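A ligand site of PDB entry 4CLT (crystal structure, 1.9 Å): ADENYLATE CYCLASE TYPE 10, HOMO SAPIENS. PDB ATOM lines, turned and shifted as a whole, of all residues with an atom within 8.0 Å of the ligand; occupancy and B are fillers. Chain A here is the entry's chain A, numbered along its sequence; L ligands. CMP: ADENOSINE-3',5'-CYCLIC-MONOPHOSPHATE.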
ATOM      1  N   TRP A 194     -29.565 -17.272 -25.980  1.00  0.00           N
ATOM      2  CA  TRP A 194     -28.432 -16.838 -25.200  1.00  0.00           C
ATOM      3  C   TRP A 194     -28.515 -17.459 -23.795  1.00  0.00           C
ATOM      4  O   TRP A 194     -27.509 -17.929 -23.253  1.00  0.00           O
ATOM      5  CB  TRP A 194     -28.403 -15.339 -25.212  1.00  0.00           C
ATOM      6  CG  TRP A 194     -27.683 -14.686 -24.102  1.00  0.00           C
ATOM      7  CD1 TRP A 194     -28.195 -13.810 -23.201  1.00  0.00           C
ATOM      8  CD2 TRP A 194     -26.278 -14.835 -23.782  1.00  0.00           C
ATOM      9  NE1 TRP A 194     -27.181 -13.392 -22.316  1.00  0.00           N
ATOM     10  CE2 TRP A 194     -26.005 -14.021 -22.667  1.00  0.00           C
ATOM     11  CE3 TRP A 194     -25.228 -15.597 -24.341  1.00  0.00           C
ATOM     12  CZ2 TRP A 194     -24.744 -13.930 -22.107  1.00  0.00           C
ATOM     13  CZ3 TRP A 194     -23.993 -15.523 -23.775  1.00  0.00           C
ATOM     14  CH2 TRP A 194     -23.757 -14.706 -22.661  1.00  0.00           C
ATOM     15  N   CYS A 197     -27.516 -21.255 -24.134  1.00  0.00           N
ATOM     16  CA  CYS A 197     -26.280 -21.633 -24.844  1.00  0.00           C
ATOM     17  C   CYS A 197     -25.158 -21.932 -23.858  1.00  0.00           C
ATOM     18  O   CYS A 197     -25.290 -21.656 -22.658  1.00  0.00           O
ATOM     19  CB  CYS A 197     -25.801 -20.553 -25.820  1.00  0.00           C
ATOM     20  SG  CYS A 197     -25.045 -19.085 -25.046  1.00  0.00           S
ATOM     21  N   ASP A 198     -24.043 -22.478 -24.404  1.00  0.00           N
ATOM     22  CA  ASP A 198     -22.859 -22.743 -23.616  1.00  0.00           C
ATOM     23  C   ASP A 198     -22.088 -21.432 -23.488  1.00  0.00           C
ATOM     24  O   ASP A 198     -21.209 -21.071 -24.287  1.00  0.00           O
ATOM     25  CB  ASP A 198     -22.020 -23.852 -24.249  1.00  0.00           C
ATOM     26  CG  ASP A 198     -20.829 -24.208 -23.405  1.00  0.00           C
ATOM     27  OD1 ASP A 198     -20.569 -23.536 -22.342  1.00  0.00           O
ATOM     28  OD2 ASP A 198     -20.106 -25.168 -23.849  1.00  0.00           O
ATOM     29  N   ARG A 199     -22.404 -20.746 -22.401  1.00  0.00           N
ATOM     30  CA  ARG A 199     -21.756 -19.499 -22.045  1.00  0.00           C
ATOM     31  C   ARG A 199     -20.263 -19.576 -21.740  1.00  0.00           C
ATOM     32  O   ARG A 199     -19.631 -18.583 -21.673  1.00  0.00           O
ATOM     33  CB  ARG A 199     -22.515 -18.884 -20.845  1.00  0.00           C
ATOM     34  CG  ARG A 199     -23.962 -18.528 -21.215  1.00  0.00           C
ATOM     35  CD  ARG A 199     -24.673 -17.723 -20.116  1.00  0.00           C
ATOM     36  NE  ARG A 199     -25.955 -17.204 -20.584  1.00  0.00           N
ATOM     37  CZ  ARG A 199     -26.753 -16.367 -19.891  1.00  0.00           C
ATOM     38  NH1 ARG A 199     -26.449 -15.951 -18.703  1.00  0.00           N
ATOM     39  NH2 ARG A 199     -27.879 -15.911 -20.444  1.00  0.00           N
ATOM     40  N   SER A 200     -19.713 -20.737 -21.486  1.00  0.00           N
ATOM     41  CA  SER A 200     -18.299 -20.846 -21.244  1.00  0.00           C
ATOM     42  C   SER A 200     -17.498 -20.743 -22.592  1.00  0.00           C
ATOM     43  O   SER A 200     -16.319 -20.447 -22.565  1.00  0.00           O
ATOM     44  CB  SER A 200     -18.021 -22.183 -20.532  1.00  0.00           C
ATOM     45  OG  SER A 200     -18.224 -23.245 -21.457  1.00  0.00           O
ATOM     46  N   MET A 201     -18.198 -20.930 -23.720  1.00  0.00           N
ATOM     47  CA  MET A 201     -17.626 -20.872 -25.076  1.00  0.00           C
ATOM     48  C   MET A 201     -18.044 -19.723 -25.959  1.00  0.00           C
ATOM     49  O   MET A 201     -17.371 -19.385 -26.879  1.00  0.00           O
ATOM     50  CB  MET A 201     -18.121 -22.054 -25.896  1.00  0.00           C
ATOM     51  CG  MET A 201     -17.599 -23.352 -25.396  1.00  0.00           C
ATOM     52  SD  MET A 201     -17.197 -24.366 -26.803  1.00  0.00           S
ATOM     53  CE  MET A 201     -17.166 -25.903 -25.902  1.00  0.00           C
ATOM     54  N   ILE A 202     -19.229 -19.198 -25.751  1.00  0.00           N
ATOM     55  CA  ILE A 202     -19.745 -18.184 -26.652  1.00  0.00           C
ATOM     56  C   ILE A 202     -19.658 -16.791 -26.057  1.00  0.00           C
ATOM     57  O   ILE A 202     -20.424 -16.480 -25.121  1.00  0.00           O
ATOM     58  CB  ILE A 202     -21.187 -18.495 -27.001  1.00  0.00           C
ATOM     59  CG1 ILE A 202     -21.277 -19.873 -27.657  1.00  0.00           C
ATOM     60  CG2 ILE A 202     -21.747 -17.433 -27.937  1.00  0.00           C
ATOM     61  CD1 ILE A 202     -22.636 -20.470 -27.439  1.00  0.00           C
ATOM     62  N   GLU A 203     -18.782 -15.970 -26.635  1.00  0.00           N
ATOM     63  CA  GLU A 203     -18.635 -14.614 -26.214  1.00  0.00           C
ATOM     64  C   GLU A 203     -19.475 -13.679 -27.011  1.00  0.00           C
ATOM     65  O   GLU A 203     -19.428 -13.698 -28.235  1.00  0.00           O
ATOM     66  CB  GLU A 203     -17.215 -14.146 -26.331  1.00  0.00           C
ATOM     67  CG  GLU A 203     -16.281 -15.025 -25.573  1.00  0.00           C
ATOM     68  CD  GLU A 203     -16.576 -14.978 -24.059  1.00  0.00           C
ATOM     69  OE1 GLU A 203     -16.612 -13.857 -23.492  1.00  0.00           O
ATOM     70  OE2 GLU A 203     -16.812 -16.070 -23.489  1.00  0.00           O
ATOM     71  N   ILE A 204     -20.208 -12.821 -26.302  1.00  0.00           N
ATOM     72  CA  ILE A 204     -21.160 -11.925 -26.886  1.00  0.00           C
ATOM     73  C   ILE A 204     -20.943 -10.491 -26.527  1.00  0.00           C
ATOM     74  O   ILE A 204     -20.044 -10.159 -25.792  1.00  0.00           O
ATOM     75  CB  ILE A 204     -22.622 -12.332 -26.544  1.00  0.00           C
ATOM     76  CG1 ILE A 204     -22.945 -12.191 -25.033  1.00  0.00           C
ATOM     77  CG2 ILE A 204     -22.833 -13.765 -27.006  1.00  0.00           C
ATOM     78  CD1 ILE A 204     -23.275 -10.802 -24.545  1.00  0.00           C
ATOM     79  N   GLU A 205     -21.796  -9.645 -27.122  1.00  0.00           N
ATOM     80  CA  GLU A 205     -21.842  -8.210 -26.880  1.00  0.00           C
ATOM     81  C   GLU A 205     -23.293  -7.849 -26.757  1.00  0.00           C
ATOM     82  O   GLU A 205     -24.151  -8.358 -27.554  1.00  0.00           O
ATOM     83  CB  GLU A 205     -21.225  -7.445 -28.029  1.00  0.00           C
ATOM     84  CG  GLU A 205     -19.937  -8.057 -28.551  1.00  0.00           C
ATOM     85  CD  GLU A 205     -19.536  -7.603 -29.970  1.00  0.00           C
ATOM     86  OE1 GLU A 205     -19.554  -6.369 -30.234  1.00  0.00           O
ATOM     87  OE2 GLU A 205     -19.173  -8.479 -30.787  1.00  0.00           O
ATOM     88  N   SER A 206     -23.600  -7.007 -25.795  1.00  0.00           N
ATOM     89  CA  SER A 206     -25.000  -6.549 -25.614  1.00  0.00           C
ATOM     90  C   SER A 206     -25.442  -5.723 -26.827  1.00  0.00           C
ATOM     91  O   SER A 206     -24.625  -5.214 -27.575  1.00  0.00           O
ATOM     92  CB  SER A 206     -25.226  -5.751 -24.341  1.00  0.00           C
ATOM     93  OG  SER A 206     -24.025  -5.184 -23.945  1.00  0.00           O
ATOM     94  N   VAL A 207     -26.749  -5.677 -27.042  1.00  0.00           N
ATOM     95  CA  VAL A 207     -27.306  -4.919 -28.137  1.00  0.00           C
ATOM     96  C   VAL A 207     -28.180  -3.931 -27.412  1.00  0.00           C
ATOM     97  O   VAL A 207     -29.041  -4.360 -26.633  1.00  0.00           O
ATOM     98  CB  VAL A 207     -28.186  -5.806 -29.057  1.00  0.00           C
ATOM     99  CG1 VAL A 207     -28.944  -4.972 -30.088  1.00  0.00           C
ATOM    100  CG2 VAL A 207     -27.342  -6.854 -29.784  1.00  0.00           C
ATOM    101  N   VAL A 213     -28.556 -10.780 -28.138  1.00  0.00           N
ATOM    102  CA  VAL A 213     -27.165 -10.449 -28.125  1.00  0.00           C
ATOM    103  C   VAL A 213     -26.503 -10.764 -29.397  1.00  0.00           C
ATOM    104  O   VAL A 213     -26.921 -11.652 -30.142  1.00  0.00           O
ATOM    105  CB  VAL A 213     -26.423 -11.146 -26.983  1.00  0.00           C
ATOM    106  CG1 VAL A 213     -26.877 -10.576 -25.570  1.00  0.00           C
ATOM    107  CG2 VAL A 213     -26.564 -12.634 -27.088  1.00  0.00           C
ATOM    108  N   LYS A 214     -25.395 -10.098 -29.600  1.00  0.00           N
ATOM    109  CA  LYS A 214     -24.574 -10.331 -30.770  1.00  0.00           C
ATOM    110  C   LYS A 214     -23.390 -11.248 -30.484  1.00  0.00           C
ATOM    111  O   LYS A 214     -22.647 -11.070 -29.503  1.00  0.00           O
ATOM    112  CB  LYS A 214     -24.114  -8.973 -31.292  1.00  0.00           C
ATOM    113  CG  LYS A 214     -23.178  -9.068 -32.466  1.00  0.00           C
ATOM    114  CD  LYS A 214     -22.684  -7.731 -32.975  1.00  0.00           C
ATOM    115  CE  LYS A 214     -21.286  -7.882 -33.537  1.00  0.00           C
ATOM    116  NZ  LYS A 214     -21.034  -6.673 -34.330  1.00  0.00           N
ATOM    117  N   ASN A 216     -19.786 -12.324 -30.658  1.00  0.00           N
ATOM    118  CA  ASN A 216     -18.487 -11.772 -30.900  1.00  0.00           C
ATOM    119  C   ASN A 216     -17.549 -12.889 -31.433  1.00  0.00           C
ATOM    120  O   ASN A 216     -17.071 -12.811 -32.538  1.00  0.00           O
ATOM    121  CB  ASN A 216     -18.008 -11.204 -29.581  1.00  0.00           C
ATOM    122  CG  ASN A 216     -16.746 -10.388 -29.722  1.00  0.00           C
ATOM    123  OD1 ASN A 216     -16.179 -10.211 -30.784  1.00  0.00           O
ATOM    124  ND2 ASN A 216     -16.256  -9.922 -28.593  1.00  0.00           N
ATOM    125  N   PHE A 217     -17.337 -13.942 -30.657  1.00  0.00           N
ATOM    126  CA  PHE A 217     -16.529 -15.063 -31.137  1.00  0.00           C
ATOM    127  C   PHE A 217     -16.733 -16.269 -30.256  1.00  0.00           C
ATOM    128  O   PHE A 217     -17.270 -16.165 -29.137  1.00  0.00           O
ATOM    129  CB  PHE A 217     -15.011 -14.704 -31.133  1.00  0.00           C
ATOM    130  CG  PHE A 217     -14.459 -14.303 -29.798  1.00  0.00           C
ATOM    131  CD1 PHE A 217     -14.530 -12.970 -29.346  1.00  0.00           C
ATOM    132  CD2 PHE A 217     -13.805 -15.236 -28.979  1.00  0.00           C
ATOM    133  CE1 PHE A 217     -13.981 -12.593 -28.121  1.00  0.00           C
ATOM    134  CE2 PHE A 217     -13.271 -14.856 -27.748  1.00  0.00           C
ATOM    135  CZ  PHE A 217     -13.359 -13.534 -27.319  1.00  0.00           C
ATOM    136  N   LYS A 219     -14.948 -19.186 -28.035  1.00  0.00           N
ATOM    137  CA  LYS A 219     -13.823 -19.276 -27.164  1.00  0.00           C
ATOM    138  C   LYS A 219     -13.686 -20.722 -26.695  1.00  0.00           C
ATOM    139  O   LYS A 219     -14.073 -21.081 -25.573  1.00  0.00           O
ATOM    140  CB  LYS A 219     -14.033 -18.353 -25.953  1.00  0.00           C
ATOM    141  CG  LYS A 219     -12.911 -18.398 -24.963  1.00  0.00           C
ATOM    142  CD  LYS A 219     -13.116 -17.435 -23.806  1.00  0.00           C
ATOM    143  CE  LYS A 219     -12.049 -17.641 -22.725  1.00  0.00           C
ATOM    144  NZ  LYS A 219     -11.361 -16.352 -22.414  1.00  0.00           N
HETATM  145  P   CMP L   1     -21.117  -6.005 -22.826  1.00  0.00           P
HETATM  146  O1P CMP L   1     -20.922  -4.532 -22.540  1.00  0.00           O
HETATM  147  O2P CMP L   1     -21.309  -6.395 -24.255  1.00  0.00           O
HETATM  148  O5' CMP L   1     -22.407  -6.441 -21.926  1.00  0.00           O
HETATM  149  C5' CMP L   1     -22.680  -7.801 -21.565  1.00  0.00           C
HETATM  150  C4' CMP L   1     -21.322  -8.405 -21.255  1.00  0.00           C
HETATM  151  O4' CMP L   1     -21.353  -9.792 -21.019  1.00  0.00           O
HETATM  152  C3' CMP L   1     -20.225  -8.274 -22.318  1.00  0.00           C
HETATM  153  O3' CMP L   1     -19.842  -6.907 -22.525  1.00  0.00           O
HETATM  154  C2' CMP L   1     -19.144  -9.110 -21.702  1.00  0.00           C
HETATM  155  O2' CMP L   1     -18.426  -8.282 -20.785  1.00  0.00           O
HETATM  156  C1' CMP L   1     -19.972 -10.186 -20.986  1.00  0.00           C
HETATM  157  N9  CMP L   1     -19.917 -11.480 -21.674  1.00  0.00           N
HETATM  158  C8  CMP L   1     -19.797 -11.724 -23.005  1.00  0.00           C
HETATM  159  N7  CMP L   1     -19.808 -13.059 -23.261  1.00  0.00           N
HETATM  160  C5  CMP L   1     -19.965 -13.684 -22.080  1.00  0.00           C
HETATM  161  C6  CMP L   1     -20.029 -15.061 -21.593  1.00  0.00           C
HETATM  162  N6  CMP L   1     -19.972 -16.131 -22.421  1.00  0.00           N
HETATM  163  N1  CMP L   1     -20.173 -15.249 -20.270  1.00  0.00           N
HETATM  164  C2  CMP L   1     -20.216 -14.245 -19.376  1.00  0.00           C
HETATM  165  N3  CMP L   1     -20.141 -12.954 -19.732  1.00  0.00           N
HETATM  166  C4  CMP L   1     -20.031 -12.630 -21.038  1.00  0.00           C
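The guanidinium group (NE) of Arg 199 lies within hydrogen-bond range of the backbone carbonyl oxygen (O) of Trp 194. OD1 of Asn 216 sits close to OE2 of Glu 205. The backbone NH (N) of Glu 205 is in hydrogen-bond range of the backbone carbonyl oxygen (O) of Lys 214 (2.9 Å). The backbone carbonyl oxygen of Glu 203 sits at hydrogen-bond distance from the backbone NH of Asn 216, at 2.8 Å. The backbone NH of Glu 203 is in hydrogen-bond range of the backbone carbonyl oxygen of Phe 217, 2.9 Å away. O of Trp 194 sits at hydrogen-bond distance from SG of Cys 197.
N6 of the ligand lies within hydrogen-bond range of O of Arg 199 (2.6 Å). N6 of the ligand is in hydrogen-bond range of O of Ile 202 (2.8 Å). N of Ser 206 lies within hydrogen-bond range of O2P of the ligand, 2.8 Å away. The side-chain hydroxyl (OG) of Ser 206 sits at hydrogen-bond distance from an oxygen (O5') of the ligand (2.9 Å). A nitrogen (N7) of the ligand sits at hydrogen-bond distance from the backbone NH (N) of Ile 204. The side-chain carboxylate (OE2) of Glu 203 sits at hydrogen-bond distance from a nitrogen (N6) of the ligand, at 3.3 Å.
Residues that only touch the ligand: Trp 194 (3.9 Å) and Glu 205 (3.2 Å). Within 4 Å of the ligand: Trp 194, Arg 199, Ile 202, Glu 203, Ile 204, Glu 205 and Ser 206. The nearest printed residue that does not touch the ligand is Ser 200 (4.7 Å).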
